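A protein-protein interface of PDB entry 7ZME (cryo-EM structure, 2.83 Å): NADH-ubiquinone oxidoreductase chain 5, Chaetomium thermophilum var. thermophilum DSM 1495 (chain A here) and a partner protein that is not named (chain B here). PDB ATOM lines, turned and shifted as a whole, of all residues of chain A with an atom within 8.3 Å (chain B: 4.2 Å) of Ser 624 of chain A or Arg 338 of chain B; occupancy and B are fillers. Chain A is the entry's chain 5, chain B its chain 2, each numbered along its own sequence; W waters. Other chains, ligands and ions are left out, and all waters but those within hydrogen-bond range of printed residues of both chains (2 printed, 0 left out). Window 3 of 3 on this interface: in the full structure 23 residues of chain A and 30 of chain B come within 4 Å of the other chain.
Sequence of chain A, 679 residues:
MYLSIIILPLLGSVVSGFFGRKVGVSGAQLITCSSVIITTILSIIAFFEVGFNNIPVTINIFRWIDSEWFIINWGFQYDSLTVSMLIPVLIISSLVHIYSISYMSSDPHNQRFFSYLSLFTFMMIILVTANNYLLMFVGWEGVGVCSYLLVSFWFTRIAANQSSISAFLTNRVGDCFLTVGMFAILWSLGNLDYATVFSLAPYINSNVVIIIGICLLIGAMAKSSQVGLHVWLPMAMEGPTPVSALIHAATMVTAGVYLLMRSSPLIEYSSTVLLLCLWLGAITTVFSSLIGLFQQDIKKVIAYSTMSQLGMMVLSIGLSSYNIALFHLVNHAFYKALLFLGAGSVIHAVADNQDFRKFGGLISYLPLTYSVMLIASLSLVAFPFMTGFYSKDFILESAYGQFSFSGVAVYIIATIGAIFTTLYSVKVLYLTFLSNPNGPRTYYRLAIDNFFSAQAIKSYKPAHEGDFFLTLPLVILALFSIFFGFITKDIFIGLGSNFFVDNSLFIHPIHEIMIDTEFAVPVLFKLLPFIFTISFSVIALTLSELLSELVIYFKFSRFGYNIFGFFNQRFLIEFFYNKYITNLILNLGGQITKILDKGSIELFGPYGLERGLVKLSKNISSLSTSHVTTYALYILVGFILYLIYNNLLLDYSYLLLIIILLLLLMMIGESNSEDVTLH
The side-chain carboxylate (OD2) of Asp 266 of chain B lies within hydrogen-bond range of the side-chain hydroxyl (OH) of Tyr 631 of chain A (2.9 Å). The side-chain amide nitrogen (NE2) of Gln 333 of chain B sits at hydrogen-bond distance from the side-chain hydroxyl (OG) of Ser 621 of chain A (3.3 Å).
N of Thr 625 of chain A lies within hydrogen-bond range of OH of Tyr 631 of chain A. The guanidinium group of Arg 338 of chain B lies within hydrogen-bond range of the side-chain amide oxygen of Gln 333 of chain B, at 3.0 Å. The guanidinium group (NH1) of Arg 338 of chain B lies within salt-bridge range of the side-chain carboxylate (OD1) of Asp 266 of chain B (3.2 Å). The backbone NH (N) of Ser 626 of chain A sits at hydrogen-bond distance from the side-chain hydroxyl (OH) of Tyr 631 of chain A (3.0 Å). O of Ser 617 of chain A sits at hydrogen-bond distance from OG of Ser 621 of chain A, at 3.0 Å.
Arg 338 of chain B touches Ser 624 of chain A. Ser 624 of chain A touches Tyr 342 of chain B (OG to OH, 3.8 Å). Asp 266 of chain B touches Ser 626 of chain A (OD2 to CB, 3.3 Å).
Of chain B, only Arg 338 and Tyr 342 come within 4 Å of Ser 624 of chain A. Printed residues of chain A within 4 Å of Arg 338 of chain B: Ser 624. Printed residues of chain B within 4 Å of Tyr 631 of chain A: Asp 266. Of the printed residues of chain B, Ser 621 of chain A touches Gln 333 (3.3 Å). Printed residues of chain A within 4 Å of Asp 266 of chain B: Ser 626 (3.3 Å) and Tyr 631 (2.9 Å). Ile 336 of chain B touches none of the printed residues of chain A. The nearest printed residue of chain B that does not touch Ser 624 of chain A is Asp 266 of chain B (4.4 Å). The nearest residue of chain A that does not touch Arg 338 of chain B is Tyr 631 of chain A (5.5 Å).
Hydrophobic or aromatic side chains of chain B within 4 Å of the printed part of chain A: Tyr 342. Hydrophobic or aromatic side chains of chain A within 4 Å of the printed part of chain B: Tyr 631. Along chain A the printed residues that touch a printed residue of chain B span positions 621 to 631. Among the printed residues, 5 pairs touch across the chains. Among the printed residues, no Asp or Glu carboxylate lies within 4 Å of a Lys or Arg side-chain nitrogen of the other chain.
Water W1 lies within hydrogen-bond range of OG of Ser 624 of chain A (2.8 Å), OH of Tyr 342 of chain B (3.0 Å) and OD1 of Asp 266 of chain B (3.1 Å). Water W2 lies within hydrogen-bond range of OH of Tyr 342 of chain B, NH2 of Arg 338 of chain B and OG of Ser 624 of chain A.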
ATOM      1  N   SER A 617     -24.304  34.108  -0.170  1.00  0.00           N
ATOM      2  CA  SER A 617     -24.923  32.841   0.202  1.00  0.00           C
ATOM      3  C   SER A 617     -24.083  31.654  -0.245  1.00  0.00           C
ATOM      4  O   SER A 617     -24.016  30.639   0.458  1.00  0.00           O
ATOM      5  CB  SER A 617     -26.324  32.753  -0.390  1.00  0.00           C
ATOM      6  OG  SER A 617     -26.281  32.796  -1.798  1.00  0.00           O
ATOM      7  N   LYS A 618     -23.453  31.751  -1.416  1.00  0.00           N
ATOM      8  CA  LYS A 618     -22.604  30.662  -1.882  1.00  0.00           C
ATOM      9  C   LYS A 618     -21.397  30.487  -0.977  1.00  0.00           C
ATOM     10  O   LYS A 618     -20.938  29.363  -0.751  1.00  0.00           O
ATOM     11  CB  LYS A 618     -22.160  30.918  -3.317  1.00  0.00           C
ATOM     12  CG  LYS A 618     -23.261  30.801  -4.337  1.00  0.00           C
ATOM     13  CD  LYS A 618     -22.701  30.444  -5.692  1.00  0.00           C
ATOM     14  CE  LYS A 618     -21.784  31.533  -6.202  1.00  0.00           C
ATOM     15  NZ  LYS A 618     -22.537  32.732  -6.631  1.00  0.00           N
ATOM     16  N   ASN A 619     -20.866  31.592  -0.456  1.00  0.00           N
ATOM     17  CA  ASN A 619     -19.719  31.514   0.437  1.00  0.00           C
ATOM     18  C   ASN A 619     -20.081  30.852   1.762  1.00  0.00           C
ATOM     19  O   ASN A 619     -19.295  30.063   2.296  1.00  0.00           O
ATOM     20  CB  ASN A 619     -19.146  32.908   0.665  1.00  0.00           C
ATOM     21  CG  ASN A 619     -18.567  33.509  -0.593  1.00  0.00           C
ATOM     22  OD1 ASN A 619     -18.537  32.871  -1.641  1.00  0.00           O
ATOM     23  ND2 ASN A 619     -18.101  34.742  -0.494  1.00  0.00           N
ATOM     24  N   ILE A 620     -21.257  31.161   2.316  1.00  0.00           N
ATOM     25  CA  ILE A 620     -21.659  30.507   3.559  1.00  0.00           C
ATOM     26  C   ILE A 620     -21.976  29.041   3.309  1.00  0.00           C
ATOM     27  O   ILE A 620     -21.767  28.194   4.185  1.00  0.00           O
ATOM     28  CB  ILE A 620     -22.849  31.233   4.208  1.00  0.00           C
ATOM     29  CG1 ILE A 620     -22.613  32.738   4.247  1.00  0.00           C
ATOM     30  CG2 ILE A 620     -23.066  30.734   5.626  1.00  0.00           C
ATOM     31  CD1 ILE A 620     -23.871  33.538   4.430  1.00  0.00           C
ATOM     32  N   SER A 621     -22.492  28.713   2.124  1.00  0.00           N
ATOM     33  CA  SER A 621     -22.681  27.315   1.761  1.00  0.00           C
ATOM     34  C   SER A 621     -21.356  26.566   1.713  1.00  0.00           C
ATOM     35  O   SER A 621     -21.323  25.351   1.931  1.00  0.00           O
ATOM     36  CB  SER A 621     -23.391  27.217   0.414  1.00  0.00           C
ATOM     37  OG  SER A 621     -24.694  27.762   0.485  1.00  0.00           O
ATOM     38  N   SER A 622     -20.258  27.271   1.430  1.00  0.00           N
ATOM     39  CA  SER A 622     -18.955  26.622   1.345  1.00  0.00           C
ATOM     40  C   SER A 622     -18.522  26.050   2.686  1.00  0.00           C
ATOM     41  O   SER A 622     -17.770  25.069   2.728  1.00  0.00           O
ATOM     42  CB  SER A 622     -17.913  27.610   0.829  1.00  0.00           C
ATOM     43  OG  SER A 622     -16.603  27.192   1.168  1.00  0.00           O
ATOM     44  N   LEU A 623     -18.981  26.681   3.769  1.00  0.00           N
ATOM     45  CA  LEU A 623     -18.615  26.240   5.134  1.00  0.00           C
ATOM     46  C   LEU A 623     -19.283  24.898   5.400  1.00  0.00           C
ATOM     47  O   LEU A 623     -18.896  24.216   6.354  1.00  0.00           O
ATOM     48  CB  LEU A 623     -19.053  27.300   6.141  1.00  0.00           C
ATOM     49  CG  LEU A 623     -18.317  28.630   6.067  1.00  0.00           C
ATOM     50  CD1 LEU A 623     -18.706  29.495   7.249  1.00  0.00           C
ATOM     51  CD2 LEU A 623     -16.816  28.406   6.046  1.00  0.00           C
ATOM     52  N   SER A 624     -20.255  24.541   4.568  1.00  0.00           N
ATOM     53  CA  SER A 624     -20.944  23.241   4.735  1.00  0.00           C
ATOM     54  C   SER A 624     -20.131  22.178   4.011  1.00  0.00           C
ATOM     55  O   SER A 624     -20.028  22.243   2.786  1.00  0.00           O
ATOM     56  CB  SER A 624     -22.383  23.307   4.292  1.00  0.00           C
ATOM     57  OG  SER A 624     -23.104  24.254   5.062  1.00  0.00           O
ATOM     58  N   THR A 625     -19.559  21.251   4.763  1.00  0.00           N
ATOM     59  CA  THR A 625     -18.655  20.231   4.190  1.00  0.00           C
ATOM     60  C   THR A 625     -19.171  18.841   4.557  1.00  0.00           C
ATOM     61  O   THR A 625     -18.635  17.871   4.002  1.00  0.00           O
ATOM     62  CB  THR A 625     -17.271  20.423   4.818  1.00  0.00           C
ATOM     63  OG1 THR A 625     -17.462  20.356   6.232  1.00  0.00           O
ATOM     64  CG2 THR A 625     -16.630  21.742   4.457  1.00  0.00           C
ATOM     65  N   SER A 626     -20.164  18.760   5.439  1.00  0.00           N
ATOM     66  CA  SER A 626     -20.665  17.456   5.942  1.00  0.00           C
ATOM     67  C   SER A 626     -19.554  16.672   6.657  1.00  0.00           C
ATOM     68  O   SER A 626     -19.652  15.436   6.726  1.00  0.00           O
ATOM     69  CB  SER A 626     -21.353  16.657   4.891  1.00  0.00           C
ATOM     70  OG  SER A 626     -22.077  15.621   5.518  1.00  0.00           O
ATOM     71  N   HIS A 627     -18.534  17.362   7.166  1.00  0.00           N
ATOM     72  CA  HIS A 627     -17.502  16.668   7.978  1.00  0.00           C
ATOM     73  C   HIS A 627     -17.782  16.969   9.450  1.00  0.00           C
ATOM     74  O   HIS A 627     -17.771  18.150   9.801  1.00  0.00           O
ATOM     75  CB  HIS A 627     -16.085  16.971   7.489  1.00  0.00           C
ATOM     76  CG  HIS A 627     -15.103  15.936   7.918  1.00  0.00           C
ATOM     77  ND1 HIS A 627     -13.853  16.256   8.407  1.00  0.00           N
ATOM     78  CD2 HIS A 627     -15.192  14.589   7.956  1.00  0.00           C
ATOM     79  CE1 HIS A 627     -13.208  15.150   8.714  1.00  0.00           C
ATOM     80  NE2 HIS A 627     -14.010  14.112   8.449  1.00  0.00           N
ATOM     81  N   THR A 630     -15.337  19.244  11.398  1.00  0.00           N
ATOM     82  CA  THR A 630     -15.470  20.681  11.050  1.00  0.00           C
ATOM     83  C   THR A 630     -16.704  21.233  11.746  1.00  0.00           C
ATOM     84  O   THR A 630     -16.643  22.362  12.247  1.00  0.00           O
ATOM     85  CB  THR A 630     -15.562  20.908   9.535  1.00  0.00           C
ATOM     86  OG1 THR A 630     -14.722  19.957   8.880  1.00  0.00           O
ATOM     87  CG2 THR A 630     -15.168  22.305   9.113  1.00  0.00           C
ATOM     88  N   TYR A 631     -17.758  20.422  11.815  1.00  0.00           N
ATOM     89  CA  TYR A 631     -19.034  20.918  12.365  1.00  0.00           C
ATOM     90  C   TYR A 631     -18.911  20.924  13.883  1.00  0.00           C
ATOM     91  O   TYR A 631     -19.520  21.791  14.511  1.00  0.00           O
ATOM     92  CB  TYR A 631     -20.152  19.999  11.879  1.00  0.00           C
ATOM     93  CG  TYR A 631     -20.628  20.219  10.467  1.00  0.00           C
ATOM     94  CD1 TYR A 631     -20.094  21.216   9.669  1.00  0.00           C
ATOM     95  CD2 TYR A 631     -21.630  19.424   9.935  1.00  0.00           C
ATOM     96  CE1 TYR A 631     -20.538  21.414   8.374  1.00  0.00           C
ATOM     97  CE2 TYR A 631     -22.086  19.610   8.643  1.00  0.00           C
ATOM     98  CZ  TYR A 631     -21.540  20.610   7.862  1.00  0.00           C
ATOM     99  OH  TYR A 631     -21.984  20.794   6.589  1.00  0.00           O
ATOM    100  N   TYR A 634     -17.102  24.151  14.511  1.00  0.00           N
ATOM    101  CA  TYR A 634     -18.027  25.276  14.424  1.00  0.00           C
ATOM    102  C   TYR A 634     -18.826  25.417  15.712  1.00  0.00           C
ATOM    103  O   TYR A 634     -18.994  26.528  16.228  1.00  0.00           O
ATOM    104  CB  TYR A 634     -18.980  25.101  13.241  1.00  0.00           C
ATOM    105  CG  TYR A 634     -18.346  25.141  11.870  1.00  0.00           C
ATOM    106  CD1 TYR A 634     -17.043  25.568  11.688  1.00  0.00           C
ATOM    107  CD2 TYR A 634     -19.065  24.748  10.754  1.00  0.00           C
ATOM    108  CE1 TYR A 634     -16.472  25.596  10.431  1.00  0.00           C
ATOM    109  CE2 TYR A 634     -18.507  24.774   9.499  1.00  0.00           C
ATOM    110  CZ  TYR A 634     -17.214  25.201   9.341  1.00  0.00           C
ATOM    111  OH  TYR A 634     -16.663  25.223   8.083  1.00  0.00           O
ATOM    112  N   PRO B 265     -29.182  20.895   7.828  1.00  0.00           N
ATOM    113  CA  PRO B 265     -29.312  20.846   6.388  1.00  0.00           C
ATOM    114  C   PRO B 265     -28.704  19.542   5.858  1.00  0.00           C
ATOM    115  O   PRO B 265     -29.298  18.949   4.985  1.00  0.00           O
ATOM    116  CB  PRO B 265     -28.531  22.098   5.962  1.00  0.00           C
ATOM    117  CG  PRO B 265     -28.650  23.020   7.140  1.00  0.00           C
ATOM    118  CD  PRO B 265     -28.493  22.088   8.316  1.00  0.00           C
ATOM    119  N   ASP B 266     -27.552  19.143   6.393  1.00  0.00           N
ATOM    120  CA  ASP B 266     -26.840  17.919   5.937  1.00  0.00           C
ATOM    121  C   ASP B 266     -27.591  16.636   6.303  1.00  0.00           C
ATOM    122  O   ASP B 266     -27.644  15.754   5.453  1.00  0.00           O
ATOM    123  CB  ASP B 266     -25.364  17.968   6.351  1.00  0.00           C
ATOM    124  CG  ASP B 266     -24.639  19.180   5.803  1.00  0.00           C
ATOM    125  OD1 ASP B 266     -25.091  20.305   6.072  1.00  0.00           O
ATOM    126  OD2 ASP B 266     -23.643  18.986   5.099  1.00  0.00           O
ATOM    127  N   ASP B 269     -31.293  16.253   4.585  1.00  0.00           N
ATOM    128  CA  ASP B 269     -31.170  15.904   3.177  1.00  0.00           C
ATOM    129  C   ASP B 269     -30.729  14.460   2.970  1.00  0.00           C
ATOM    130  O   ASP B 269     -31.010  13.887   1.914  1.00  0.00           O
ATOM    131  CB  ASP B 269     -30.188  16.860   2.502  1.00  0.00           C
ATOM    132  CG  ASP B 269     -30.335  16.889   1.001  1.00  0.00           C
ATOM    133  OD1 ASP B 269     -31.480  16.930   0.511  1.00  0.00           O
ATOM    134  OD2 ASP B 269     -29.298  16.880   0.310  1.00  0.00           O
ATOM    135  N   GLN B 333     -29.731  27.331  -2.487  1.00  0.00           N
ATOM    136  CA  GLN B 333     -29.988  25.884  -2.260  1.00  0.00           C
ATOM    137  C   GLN B 333     -30.801  25.313  -3.427  1.00  0.00           C
ATOM    138  O   GLN B 333     -31.897  25.826  -3.676  1.00  0.00           O
ATOM    139  CB  GLN B 333     -30.697  25.691  -0.919  1.00  0.00           C
ATOM    140  CG  GLN B 333     -29.867  26.120   0.281  1.00  0.00           C
ATOM    141  CD  GLN B 333     -28.572  25.356   0.416  1.00  0.00           C
ATOM    142  OE1 GLN B 333     -28.565  24.158   0.681  1.00  0.00           O
ATOM    143  NE2 GLN B 333     -27.460  26.052   0.250  1.00  0.00           N
ATOM    144  N   ARG B 335     -31.299  21.974  -3.647  1.00  0.00           N
ATOM    145  CA  ARG B 335     -31.885  20.719  -3.116  1.00  0.00           C
ATOM    146  C   ARG B 335     -33.115  21.082  -2.279  1.00  0.00           C
ATOM    147  O   ARG B 335     -32.974  21.915  -1.385  1.00  0.00           O
ATOM    148  CB  ARG B 335     -30.774  19.872  -2.493  1.00  0.00           C
ATOM    149  CG  ARG B 335     -29.805  19.310  -3.519  1.00  0.00           C
ATOM    150  CD  ARG B 335     -28.826  18.305  -2.958  1.00  0.00           C
ATOM    151  NE  ARG B 335     -29.507  17.202  -2.304  1.00  0.00           N
ATOM    152  CZ  ARG B 335     -29.913  16.091  -2.903  1.00  0.00           C
ATOM    153  NH1 ARG B 335     -30.522  15.154  -2.201  1.00  0.00           N
ATOM    154  NH2 ARG B 335     -29.713  15.921  -4.195  1.00  0.00           N
ATOM    155  N   ILE B 336     -34.262  20.474  -2.567  1.00  0.00           N
ATOM    156  CA  ILE B 336     -35.553  20.834  -1.907  1.00  0.00           C
ATOM    157  C   ILE B 336     -35.481  20.644  -0.387  1.00  0.00           C
ATOM    158  O   ILE B 336     -35.983  21.515   0.326  1.00  0.00           O
ATOM    159  CB  ILE B 336     -36.721  20.046  -2.543  1.00  0.00           C
ATOM    160  CG1 ILE B 336     -38.083  20.543  -2.050  1.00  0.00           C
ATOM    161  CG2 ILE B 336     -36.573  18.543  -2.375  1.00  0.00           C
ATOM    162  CD1 ILE B 336     -38.370  21.989  -2.385  1.00  0.00           C
ATOM    163  N   LYS B 337     -34.890  19.546   0.080  1.00  0.00           N
ATOM    164  CA  LYS B 337     -34.786  19.287   1.539  1.00  0.00           C
ATOM    165  C   LYS B 337     -33.654  20.068   2.208  1.00  0.00           C
ATOM    166  O   LYS B 337     -33.728  20.265   3.430  1.00  0.00           O
ATOM    167  CB  LYS B 337     -34.715  17.780   1.783  1.00  0.00           C
ATOM    168  CG  LYS B 337     -35.988  17.033   1.405  1.00  0.00           C
ATOM    169  CD  LYS B 337     -35.809  15.544   1.239  1.00  0.00           C
ATOM    170  CE  LYS B 337     -35.268  14.883   2.484  1.00  0.00           C
ATOM    171  NZ  LYS B 337     -34.911  13.468   2.244  1.00  0.00           N
ATOM    172  N   ARG B 338     -32.655  20.507   1.447  1.00  0.00           N
ATOM    173  CA  ARG B 338     -31.604  21.377   2.021  1.00  0.00           C
ATOM    174  C   ARG B 338     -32.249  22.751   2.191  1.00  0.00           C
ATOM    175  O   ARG B 338     -31.788  23.525   3.040  1.00  0.00           O
ATOM    176  CB  ARG B 338     -30.341  21.358   1.154  1.00  0.00           C
ATOM    177  CG  ARG B 338     -29.416  20.184   1.416  1.00  0.00           C
ATOM    178  CD  ARG B 338     -28.022  20.456   0.894  1.00  0.00           C
ATOM    179  NE  ARG B 338     -27.382  21.532   1.635  1.00  0.00           N
ATOM    180  CZ  ARG B 338     -26.584  21.355   2.680  1.00  0.00           C
ATOM    181  NH1 ARG B 338     -26.322  20.134   3.110  1.00  0.00           N
ATOM    182  NH2 ARG B 338     -26.052  22.397   3.287  1.00  0.00           N
ATOM    183  N   LEU B 339     -33.336  22.994   1.459  1.00  0.00           N
ATOM    184  CA  LEU B 339     -34.000  24.318   1.469  1.00  0.00           C
ATOM    185  C   LEU B 339     -35.018  24.377   2.604  1.00  0.00           C
ATOM    186  O   LEU B 339     -35.123  25.428   3.247  1.00  0.00           O
ATOM    187  CB  LEU B 339     -34.694  24.536   0.124  1.00  0.00           C
ATOM    188  CG  LEU B 339     -35.349  25.907  -0.026  1.00  0.00           C
ATOM    189  CD1 LEU B 339     -34.290  26.989  -0.075  1.00  0.00           C
ATOM    190  CD2 LEU B 339     -36.237  25.969  -1.253  1.00  0.00           C
ATOM    191  N   LEU B 340     -35.735  23.281   2.824  1.00  0.00           N
ATOM    192  CA  LEU B 340     -36.690  23.246   3.923  1.00  0.00           C
ATOM    193  C   LEU B 340     -36.007  23.404   5.272  1.00  0.00           C
ATOM    194  O   LEU B 340     -36.557  24.053   6.166  1.00  0.00           O
ATOM    195  CB  LEU B 340     -37.480  21.944   3.879  1.00  0.00           C
ATOM    196  CG  LEU B 340     -38.431  21.811   2.693  1.00  0.00           C
ATOM    197  CD1 LEU B 340     -38.551  20.361   2.291  1.00  0.00           C
ATOM    198  CD2 LEU B 340     -39.788  22.387   3.030  1.00  0.00           C
ATOM    199  N   ALA B 341     -34.812  22.840   5.428  1.00  0.00           N
ATOM    200  CA  ALA B 341     -34.070  22.979   6.697  1.00  0.00           C
ATOM    201  C   ALA B 341     -33.715  24.445   6.946  1.00  0.00           C
ATOM    202  O   ALA B 341     -33.926  24.899   8.072  1.00  0.00           O
ATOM    203  CB  ALA B 341     -32.855  22.108   6.654  1.00  0.00           C
ATOM    204  N   TYR B 342     -33.234  25.163   5.932  1.00  0.00           N
ATOM    205  CA  TYR B 342     -32.838  26.589   6.059  1.00  0.00           C
ATOM    206  C   TYR B 342     -34.075  27.434   6.333  1.00  0.00           C
ATOM    207  O   TYR B 342     -33.968  28.457   7.015  1.00  0.00           O
ATOM    208  CB  TYR B 342     -31.990  27.030   4.864  1.00  0.00           C
ATOM    209  CG  TYR B 342     -30.530  26.700   5.019  1.00  0.00           C
ATOM    210  CD1 TYR B 342     -29.783  27.261   6.040  1.00  0.00           C
ATOM    211  CD2 TYR B 342     -29.902  25.815   4.161  1.00  0.00           C
ATOM    212  CE1 TYR B 342     -28.444  26.951   6.205  1.00  0.00           C
ATOM    213  CE2 TYR B 342     -28.564  25.498   4.309  1.00  0.00           C
ATOM    214  CZ  TYR B 342     -27.834  26.066   5.336  1.00  0.00           C
ATOM    215  OH  TYR B 342     -26.514  25.761   5.488  1.00  0.00           O
HETATM  216  O   HOH W   1     -25.225  23.346   6.651  1.00  0.00           O
HETATM  217  O   HOH W   2     -25.055  25.171   2.992  1.00  0.00           O
